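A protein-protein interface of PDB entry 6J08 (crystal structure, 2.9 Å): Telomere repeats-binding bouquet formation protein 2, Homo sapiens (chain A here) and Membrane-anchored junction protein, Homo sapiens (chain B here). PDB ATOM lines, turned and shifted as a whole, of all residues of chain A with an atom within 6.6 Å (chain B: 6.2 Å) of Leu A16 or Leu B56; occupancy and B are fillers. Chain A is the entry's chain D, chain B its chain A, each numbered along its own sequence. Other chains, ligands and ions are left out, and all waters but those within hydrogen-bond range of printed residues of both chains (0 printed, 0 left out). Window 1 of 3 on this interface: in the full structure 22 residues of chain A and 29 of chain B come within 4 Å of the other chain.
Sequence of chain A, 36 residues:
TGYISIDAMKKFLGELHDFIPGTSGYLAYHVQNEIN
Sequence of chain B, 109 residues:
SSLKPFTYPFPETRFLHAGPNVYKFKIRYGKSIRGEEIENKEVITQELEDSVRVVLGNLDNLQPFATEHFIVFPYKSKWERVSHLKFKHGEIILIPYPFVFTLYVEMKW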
ATOM      1  N   LYS A  10      17.555   1.274  -9.199  1.00  0.00           N
ATOM      2  CA  LYS A  10      18.779   0.438  -9.227  1.00  0.00           C
ATOM      3  C   LYS A  10      19.890   1.283  -9.855  1.00  0.00           C
ATOM      4  O   LYS A  10      19.564   2.158 -10.683  1.00  0.00           O
ATOM      5  CB  LYS A  10      18.511  -0.879  -9.962  1.00  0.00           C
ATOM      6  CG  LYS A  10      18.230  -0.771 -11.451  1.00  0.00           C
ATOM      7  CD  LYS A  10      17.808  -2.084 -12.084  1.00  0.00           C
ATOM      8  CE  LYS A  10      17.305  -1.885 -13.499  1.00  0.00           C
ATOM      9  NZ  LYS A  10      16.655  -3.106 -14.022  1.00  0.00           N
ATOM     10  N   LYS A  11      21.149   1.070  -9.457  1.00  0.00           N
ATOM     11  CA  LYS A  11      22.276   1.908  -9.944  1.00  0.00           C
ATOM     12  C   LYS A  11      23.535   1.082 -10.219  1.00  0.00           C
ATOM     13  O   LYS A  11      23.669  -0.002  -9.705  1.00  0.00           O
ATOM     14  CB  LYS A  11      22.529   3.049  -8.957  1.00  0.00           C
ATOM     15  CG  LYS A  11      22.841   2.667  -7.522  1.00  0.00           C
ATOM     16  CD  LYS A  11      22.787   3.887  -6.634  1.00  0.00           C
ATOM     17  CE  LYS A  11      23.250   3.660  -5.214  1.00  0.00           C
ATOM     18  NZ  LYS A  11      23.261   4.932  -4.452  1.00  0.00           N
ATOM     19  N   PHE A  12      24.415   1.606 -11.056  1.00  0.00           N
ATOM     20  CA  PHE A  12      25.754   1.041 -11.336  1.00  0.00           C
ATOM     21  C   PHE A  12      26.629   1.138 -10.079  1.00  0.00           C
ATOM     22  O   PHE A  12      26.832   2.262  -9.553  1.00  0.00           O
ATOM     23  CB  PHE A  12      26.393   1.803 -12.491  1.00  0.00           C
ATOM     24  CG  PHE A  12      27.852   1.519 -12.691  1.00  0.00           C
ATOM     25  CD1 PHE A  12      28.251   0.373 -13.350  1.00  0.00           C
ATOM     26  CD2 PHE A  12      28.816   2.402 -12.230  1.00  0.00           C
ATOM     27  CE1 PHE A  12      29.596   0.120 -13.561  1.00  0.00           C
ATOM     28  CE2 PHE A  12      30.161   2.140 -12.431  1.00  0.00           C
ATOM     29  CZ  PHE A  12      30.546   1.001 -13.104  1.00  0.00           C
ATOM     30  N   GLY A  14      29.931  -0.065  -9.764  1.00  0.00           N
ATOM     31  CA  GLY A  14      31.337  -0.392 -10.040  1.00  0.00           C
ATOM     32  C   GLY A  14      32.258   0.784  -9.784  1.00  0.00           C
ATOM     33  O   GLY A  14      31.764   1.901  -9.533  1.00  0.00           O
ATOM     34  N   GLU A  15      33.563   0.539  -9.856  1.00  0.00           N
ATOM     35  CA  GLU A  15      34.567   1.617  -9.970  1.00  0.00           C
ATOM     36  C   GLU A  15      34.089   2.588 -11.054  1.00  0.00           C
ATOM     37  O   GLU A  15      33.576   2.129 -12.103  1.00  0.00           O
ATOM     38  CB  GLU A  15      35.948   1.046 -10.288  1.00  0.00           C
ATOM     39  CG  GLU A  15      36.644   0.454  -9.080  1.00  0.00           C
ATOM     40  CD  GLU A  15      38.114   0.139  -9.294  1.00  0.00           C
ATOM     41  OE1 GLU A  15      38.675   0.618 -10.303  1.00  0.00           O
ATOM     42  OE2 GLU A  15      38.698  -0.589  -8.452  1.00  0.00           O
ATOM     43  N   LEU A  16      34.279   3.876 -10.788  1.00  0.00           N
ATOM     44  CA  LEU A  16      33.814   5.016 -11.609  1.00  0.00           C
ATOM     45  C   LEU A  16      34.852   6.127 -11.435  1.00  0.00           C
ATOM     46  O   LEU A  16      35.119   6.518 -10.297  1.00  0.00           O
ATOM     47  CB  LEU A  16      32.415   5.419 -11.120  1.00  0.00           C
ATOM     48  CG  LEU A  16      31.729   6.591 -11.823  1.00  0.00           C
ATOM     49  CD1 LEU A  16      31.443   6.283 -13.285  1.00  0.00           C
ATOM     50  CD2 LEU A  16      30.429   6.935 -11.120  1.00  0.00           C
ATOM     51  N   HIS A  17      35.450   6.585 -12.526  1.00  0.00           N
ATOM     52  CA  HIS A  17      36.537   7.595 -12.526  1.00  0.00           C
ATOM     53  C   HIS A  17      36.178   8.720 -13.493  1.00  0.00           C
ATOM     54  O   HIS A  17      35.515   8.433 -14.510  1.00  0.00           O
ATOM     55  CB  HIS A  17      37.852   6.934 -12.925  1.00  0.00           C
ATOM     56  CG  HIS A  17      38.112   5.661 -12.207  1.00  0.00           C
ATOM     57  ND1 HIS A  17      38.761   5.628 -10.991  1.00  0.00           N
ATOM     58  CD2 HIS A  17      37.822   4.382 -12.531  1.00  0.00           C
ATOM     59  CE1 HIS A  17      38.875   4.380 -10.588  1.00  0.00           C
ATOM     60  NE2 HIS A  17      38.304   3.591 -11.518  1.00  0.00           N
ATOM     61  N   ASP A  18      36.601   9.941 -13.177  1.00  0.00           N
ATOM     62  CA  ASP A  18      36.607  11.076 -14.134  1.00  0.00           C
ATOM     63  C   ASP A  18      37.646  10.794 -15.217  1.00  0.00           C
ATOM     64  O   ASP A  18      38.852  10.696 -14.891  1.00  0.00           O
ATOM     65  CB  ASP A  18      36.956  12.404 -13.468  1.00  0.00           C
ATOM     66  CG  ASP A  18      35.945  12.800 -12.421  1.00  0.00           C
ATOM     67  OD1 ASP A  18      34.821  13.177 -12.817  1.00  0.00           O
ATOM     68  OD2 ASP A  18      36.280  12.682 -11.228  1.00  0.00           O
ATOM     69  N   LEU B   3      34.339  10.427  -6.376  1.00  0.00           N
ATOM     70  CA  LEU B   3      35.326  10.990  -7.342  1.00  0.00           C
ATOM     71  C   LEU B   3      35.128  12.519  -7.345  1.00  0.00           C
ATOM     72  O   LEU B   3      34.474  13.012  -6.411  1.00  0.00           O
ATOM     73  CB  LEU B   3      34.997  10.496  -8.760  1.00  0.00           C
ATOM     74  CG  LEU B   3      33.529  10.471  -9.208  1.00  0.00           C
ATOM     75  CD1 LEU B   3      32.931  11.862  -9.355  1.00  0.00           C
ATOM     76  CD2 LEU B   3      33.406   9.720 -10.520  1.00  0.00           C
ATOM     77  N   LEU B  16      33.308  10.151 -18.041  1.00  0.00           N
ATOM     78  CA  LEU B  16      33.350   9.151 -16.959  1.00  0.00           C
ATOM     79  C   LEU B  16      33.761   7.812 -17.536  1.00  0.00           C
ATOM     80  O   LEU B  16      33.199   7.403 -18.542  1.00  0.00           O
ATOM     81  CB  LEU B  16      31.981   9.092 -16.295  1.00  0.00           C
ATOM     82  CG  LEU B  16      31.595  10.380 -15.577  1.00  0.00           C
ATOM     83  CD1 LEU B  16      30.181  10.285 -15.048  1.00  0.00           C
ATOM     84  CD2 LEU B  16      32.562  10.687 -14.449  1.00  0.00           C
ATOM     85  N   HIS B  17      34.780   7.226 -16.925  1.00  0.00           N
ATOM     86  CA  HIS B  17      35.272   5.866 -17.214  1.00  0.00           C
ATOM     87  C   HIS B  17      34.504   4.933 -16.296  1.00  0.00           C
ATOM     88  O   HIS B  17      34.616   5.132 -15.081  1.00  0.00           O
ATOM     89  CB  HIS B  17      36.782   5.815 -16.987  1.00  0.00           C
ATOM     90  CG  HIS B  17      37.386   4.497 -17.300  1.00  0.00           C
ATOM     91  ND1 HIS B  17      38.592   4.117 -16.785  1.00  0.00           N
ATOM     92  CD2 HIS B  17      36.942   3.470 -18.056  1.00  0.00           C
ATOM     93  CE1 HIS B  17      38.881   2.907 -17.221  1.00  0.00           C
ATOM     94  NE2 HIS B  17      37.882   2.487 -18.010  1.00  0.00           N
ATOM     95  N   ALA B  18      33.701   4.021 -16.842  1.00  0.00           N
ATOM     96  CA  ALA B  18      32.966   3.032 -16.028  1.00  0.00           C
ATOM     97  C   ALA B  18      32.846   1.734 -16.804  1.00  0.00           C
ATOM     98  O   ALA B  18      32.398   1.781 -17.961  1.00  0.00           O
ATOM     99  CB  ALA B  18      31.622   3.568 -15.667  1.00  0.00           C
ATOM    100  N   TYR B  23      31.499   7.482 -20.808  1.00  0.00           N
ATOM    101  CA  TYR B  23      30.176   8.142 -20.847  1.00  0.00           C
ATOM    102  C   TYR B  23      30.388   9.659 -20.898  1.00  0.00           C
ATOM    103  O   TYR B  23      31.150  10.182 -20.093  1.00  0.00           O
ATOM    104  CB  TYR B  23      29.326   7.672 -19.665  1.00  0.00           C
ATOM    105  CG  TYR B  23      29.039   6.196 -19.664  1.00  0.00           C
ATOM    106  CD1 TYR B  23      29.941   5.306 -19.118  1.00  0.00           C
ATOM    107  CD2 TYR B  23      27.880   5.681 -20.225  1.00  0.00           C
ATOM    108  CE1 TYR B  23      29.686   3.947 -19.089  1.00  0.00           C
ATOM    109  CE2 TYR B  23      27.621   4.319 -20.228  1.00  0.00           C
ATOM    110  CZ  TYR B  23      28.531   3.452 -19.656  1.00  0.00           C
ATOM    111  OH  TYR B  23      28.298   2.115 -19.630  1.00  0.00           O
ATOM    112  N   PHE B  25      28.631  12.951 -19.936  1.00  0.00           N
ATOM    113  CA  PHE B  25      27.567  13.554 -19.102  1.00  0.00           C
ATOM    114  C   PHE B  25      27.644  15.069 -19.221  1.00  0.00           C
ATOM    115  O   PHE B  25      28.757  15.599 -19.166  1.00  0.00           O
ATOM    116  CB  PHE B  25      27.724  13.124 -17.648  1.00  0.00           C
ATOM    117  CG  PHE B  25      27.061  11.811 -17.362  1.00  0.00           C
ATOM    118  CD1 PHE B  25      27.622  10.635 -17.813  1.00  0.00           C
ATOM    119  CD2 PHE B  25      25.854  11.759 -16.692  1.00  0.00           C
ATOM    120  CE1 PHE B  25      26.989   9.424 -17.594  1.00  0.00           C
ATOM    121  CE2 PHE B  25      25.227  10.550 -16.465  1.00  0.00           C
ATOM    122  CZ  PHE B  25      25.790   9.383 -16.926  1.00  0.00           C
ATOM    123  N   GLU B  49      26.847  12.083  -7.838  1.00  0.00           N
ATOM    124  CA  GLU B  49      27.447  10.774  -8.163  1.00  0.00           C
ATOM    125  C   GLU B  49      26.355   9.710  -8.096  1.00  0.00           C
ATOM    126  O   GLU B  49      26.277   8.916  -9.029  1.00  0.00           O
ATOM    127  CB  GLU B  49      28.572  10.407  -7.209  1.00  0.00           C
ATOM    128  CG  GLU B  49      29.269   9.126  -7.622  1.00  0.00           C
ATOM    129  CD  GLU B  49      30.355   8.676  -6.662  1.00  0.00           C
ATOM    130  OE1 GLU B  49      30.995   9.565  -6.055  1.00  0.00           O
ATOM    131  OE2 GLU B  49      30.544   7.438  -6.513  1.00  0.00           O
ATOM    132  N   SER B  51      23.228  10.057  -8.462  1.00  0.00           N
ATOM    133  CA  SER B  51      22.460  10.440  -9.675  1.00  0.00           C
ATOM    134  C   SER B  51      23.114   9.825 -10.927  1.00  0.00           C
ATOM    135  O   SER B  51      22.405   9.187 -11.729  1.00  0.00           O
ATOM    136  CB  SER B  51      22.341  11.939  -9.780  1.00  0.00           C
ATOM    137  OG  SER B  51      21.469  12.437  -8.776  1.00  0.00           O
ATOM    138  N   VAL B  52      24.425   9.977 -11.094  1.00  0.00           N
ATOM    139  CA  VAL B  52      25.117   9.426 -12.286  1.00  0.00           C
ATOM    140  C   VAL B  52      24.948   7.897 -12.296  1.00  0.00           C
ATOM    141  O   VAL B  52      24.544   7.339 -13.341  1.00  0.00           O
ATOM    142  CB  VAL B  52      26.598   9.837 -12.332  1.00  0.00           C
ATOM    143  CG1 VAL B  52      27.338   9.070 -13.412  1.00  0.00           C
ATOM    144  CG2 VAL B  52      26.774  11.325 -12.553  1.00  0.00           C
ATOM    145  N   ARG B  53      25.266   7.235 -11.188  1.00  0.00           N
ATOM    146  CA  ARG B  53      25.238   5.753 -11.069  1.00  0.00           C
ATOM    147  C   ARG B  53      23.846   5.255 -11.452  1.00  0.00           C
ATOM    148  O   ARG B  53      23.724   4.152 -11.993  1.00  0.00           O
ATOM    149  CB  ARG B  53      25.566   5.314  -9.639  1.00  0.00           C
ATOM    150  CG  ARG B  53      27.027   5.513  -9.272  1.00  0.00           C
ATOM    151  CD  ARG B  53      27.406   4.917  -7.934  1.00  0.00           C
ATOM    152  NE  ARG B  53      28.839   5.103  -7.774  1.00  0.00           N
ATOM    153  CZ  ARG B  53      29.786   4.238  -8.130  1.00  0.00           C
ATOM    154  NH1 ARG B  53      29.495   3.063  -8.655  1.00  0.00           N
ATOM    155  NH2 ARG B  53      31.045   4.556  -7.944  1.00  0.00           N
ATOM    156  N   VAL B  54      22.825   6.046 -11.143  1.00  0.00           N
ATOM    157  CA  VAL B  54      21.409   5.657 -11.366  1.00  0.00           C
ATOM    158  C   VAL B  54      21.167   5.610 -12.870  1.00  0.00           C
ATOM    159  O   VAL B  54      20.674   4.597 -13.356  1.00  0.00           O
ATOM    160  CB  VAL B  54      20.484   6.638 -10.635  1.00  0.00           C
ATOM    161  CG1 VAL B  54      19.081   6.648 -11.208  1.00  0.00           C
ATOM    162  CG2 VAL B  54      20.473   6.304  -9.157  1.00  0.00           C
ATOM    163  N   VAL B  55      21.498   6.700 -13.548  1.00  0.00           N
ATOM    164  CA  VAL B  55      21.438   6.826 -15.024  1.00  0.00           C
ATOM    165  C   VAL B  55      22.242   5.674 -15.627  1.00  0.00           C
ATOM    166  O   VAL B  55      21.716   4.991 -16.535  1.00  0.00           O
ATOM    167  CB  VAL B  55      22.003   8.180 -15.467  1.00  0.00           C
ATOM    168  CG1 VAL B  55      22.256   8.193 -16.959  1.00  0.00           C
ATOM    169  CG2 VAL B  55      21.088   9.319 -15.070  1.00  0.00           C
ATOM    170  N   LEU B  56      23.468   5.450 -15.128  1.00  0.00           N
ATOM    171  CA  LEU B  56      24.399   4.436 -15.698  1.00  0.00           C
ATOM    172  C   LEU B  56      23.775   3.058 -15.547  1.00  0.00           C
ATOM    173  O   LEU B  56      24.038   2.222 -16.388  1.00  0.00           O
ATOM    174  CB  LEU B  56      25.760   4.494 -15.004  1.00  0.00           C
ATOM    175  CG  LEU B  56      26.691   5.631 -15.431  1.00  0.00           C
ATOM    176  CD1 LEU B  56      27.993   5.541 -14.668  1.00  0.00           C
ATOM    177  CD2 LEU B  56      26.976   5.621 -16.929  1.00  0.00           C
ATOM    178  N   GLY B  57      22.959   2.864 -14.526  1.00  0.00           N
ATOM    179  CA  GLY B  57      22.231   1.613 -14.270  1.00  0.00           C
ATOM    180  C   GLY B  57      20.824   1.572 -14.874  1.00  0.00           C
ATOM    181  O   GLY B  57      20.109   0.572 -14.608  1.00  0.00           O
ATOM    182  N   ASN B  58      20.398   2.574 -15.646  1.00  0.00           N
ATOM    183  CA  ASN B  58      19.038   2.545 -16.265  1.00  0.00           C
ATOM    184  C   ASN B  58      19.080   3.203 -17.653  1.00  0.00           C
ATOM    185  O   ASN B  58      18.145   3.957 -17.998  1.00  0.00           O
ATOM    186  CB  ASN B  58      17.979   3.169 -15.349  1.00  0.00           C
ATOM    187  CG  ASN B  58      17.856   2.470 -14.010  1.00  0.00           C
ATOM    188  OD1 ASN B  58      17.005   1.595 -13.825  1.00  0.00           O
ATOM    189  ND2 ASN B  58      18.706   2.849 -13.066  1.00  0.00           N
ATOM    190  N   LEU B  59      20.105   2.866 -18.439  1.00  0.00           N
ATOM    191  CA  LEU B  59      20.514   3.593 -19.667  1.00  0.00           C
ATOM    192  C   LEU B  59      19.342   3.667 -20.632  1.00  0.00           C
ATOM    193  O   LEU B  59      19.255   4.664 -21.358  1.00  0.00           O
ATOM    194  CB  LEU B  59      21.665   2.840 -20.328  1.00  0.00           C
ATOM    195  CG  LEU B  59      22.967   2.792 -19.549  1.00  0.00           C
ATOM    196  CD1 LEU B  59      23.920   1.838 -20.236  1.00  0.00           C
ATOM    197  CD2 LEU B  59      23.581   4.178 -19.429  1.00  0.00           C
ATOM    198  N   PHE B 101      24.315  11.950 -22.077  1.00  0.00           N
ATOM    199  CA  PHE B 101      23.363  12.120 -20.954  1.00  0.00           C
ATOM    200  C   PHE B 101      23.409  13.567 -20.483  1.00  0.00           C
ATOM    201  O   PHE B 101      24.470  14.012 -20.042  1.00  0.00           O
ATOM    202  CB  PHE B 101      23.671  11.130 -19.832  1.00  0.00           C
ATOM    203  CG  PHE B 101      23.421   9.714 -20.266  1.00  0.00           C
ATOM    204  CD1 PHE B 101      24.464   8.918 -20.707  1.00  0.00           C
ATOM    205  CD2 PHE B 101      22.131   9.222 -20.338  1.00  0.00           C
ATOM    206  CE1 PHE B 101      24.222   7.629 -21.151  1.00  0.00           C
ATOM    207  CE2 PHE B 101      21.893   7.940 -20.795  1.00  0.00           C
ATOM    208  CZ  PHE B 101      22.937   7.143 -21.182  1.00  0.00           C
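N of His B17 lies within hydrogen-bond range of O of His A17.
O of Arg B53 lies within hydrogen-bond range of N of Phe A12 (2.8 Å).
The backbone carbonyl oxygen (O) of Gly A14 sits at hydrogen-bond distance from the guanidinium group (NH1) of Arg B53 (2.7 Å).
The backbone carbonyl oxygen (O) of Lys A10 is in hydrogen-bond range of the side-chain amide nitrogen (ND2) of Asn B58, 2.6 Å away.
The side-chain carboxylate (OE1) of Glu B49 sits at hydrogen-bond distance from the backbone NH (N) of Leu B3, at 3.5 Å.
The backbone carbonyl oxygen (O) of Leu B16 lies within hydrogen-bond range of the backbone NH (N) of Tyr B23, 2.8 Å away.
The side-chain carboxylate (OE2) of Glu B49 is in salt-bridge range of the guanidinium group (NE) of Arg B53 (3.2 Å).
ND2 of Asn B58 sits at hydrogen-bond distance from O of Val B54 (2.6 Å).
The side-chain carboxylate (OE1) of Glu A15 is in hydrogen-bond range of a ring nitrogen (NE2) of His A17.
O of Lys A10 touches O of Val B54, 3.8 Å away.
CE of Lys A10 touches O of Gly B57 (3.9 Å).
Arg B53 touches Lys A11 (O to CA, 3.4 Å).
Lys A11 touches Val B54.
CZ of Phe A12 touches CB of Ala B18 (3.8 Å).
CB of Phe A12 touches CB of Leu B56 (3.7 Å).
Phe A12 touches Gly B57.
Leu A16 touches His B17.
Asp A18 touches Leu B3 (OD2 to CB, 3.5 Å).
CD2 of Leu B16 touches OD1 of Asp A18, 3.7 Å away.
Printed residues of chain B within 4 Å of Leu A16: Leu B3, His B17, Ala B18, Arg B53 and Leu B56.
Leu B56 touches just these residues of chain A: Phe A12 (3.7 Å) and Leu A16 (3.8 Å).
Of the printed residues of chain B, Phe A12 touches Ala B18 (3.8 Å), Arg B53 (2.8 Å), Leu B56 (3.7 Å) and Gly B57 (3.9 Å).
Of the printed residues of chain B, His A17 touches Leu B16 and His B17.
Printed residues of chain A within 4 Å of Ala B18: Phe A12 (3.8 Å) and Leu A16 (3.6 Å).
Of the printed residues of chain B, Gly A14 touches Arg B53.
The nearest residue of chain A that does not touch Leu B56 is Lys A11 (5.7 Å).
The nearest printed residue of chain A that does not touch Asn B58 is Lys A11 (4.7 Å).
Printed residues of chain A that touch a printed residue of chain B: Lys A10, Lys A11, Phe A12, Gly A14, Leu A16, His A17 and Asp A18.
Among the printed residues, 19 pairs touch across the chains.
Among the printed residues, no Asp or Glu carboxylate lies within 4 Å of a Lys or Arg side-chain nitrogen of the other chain.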
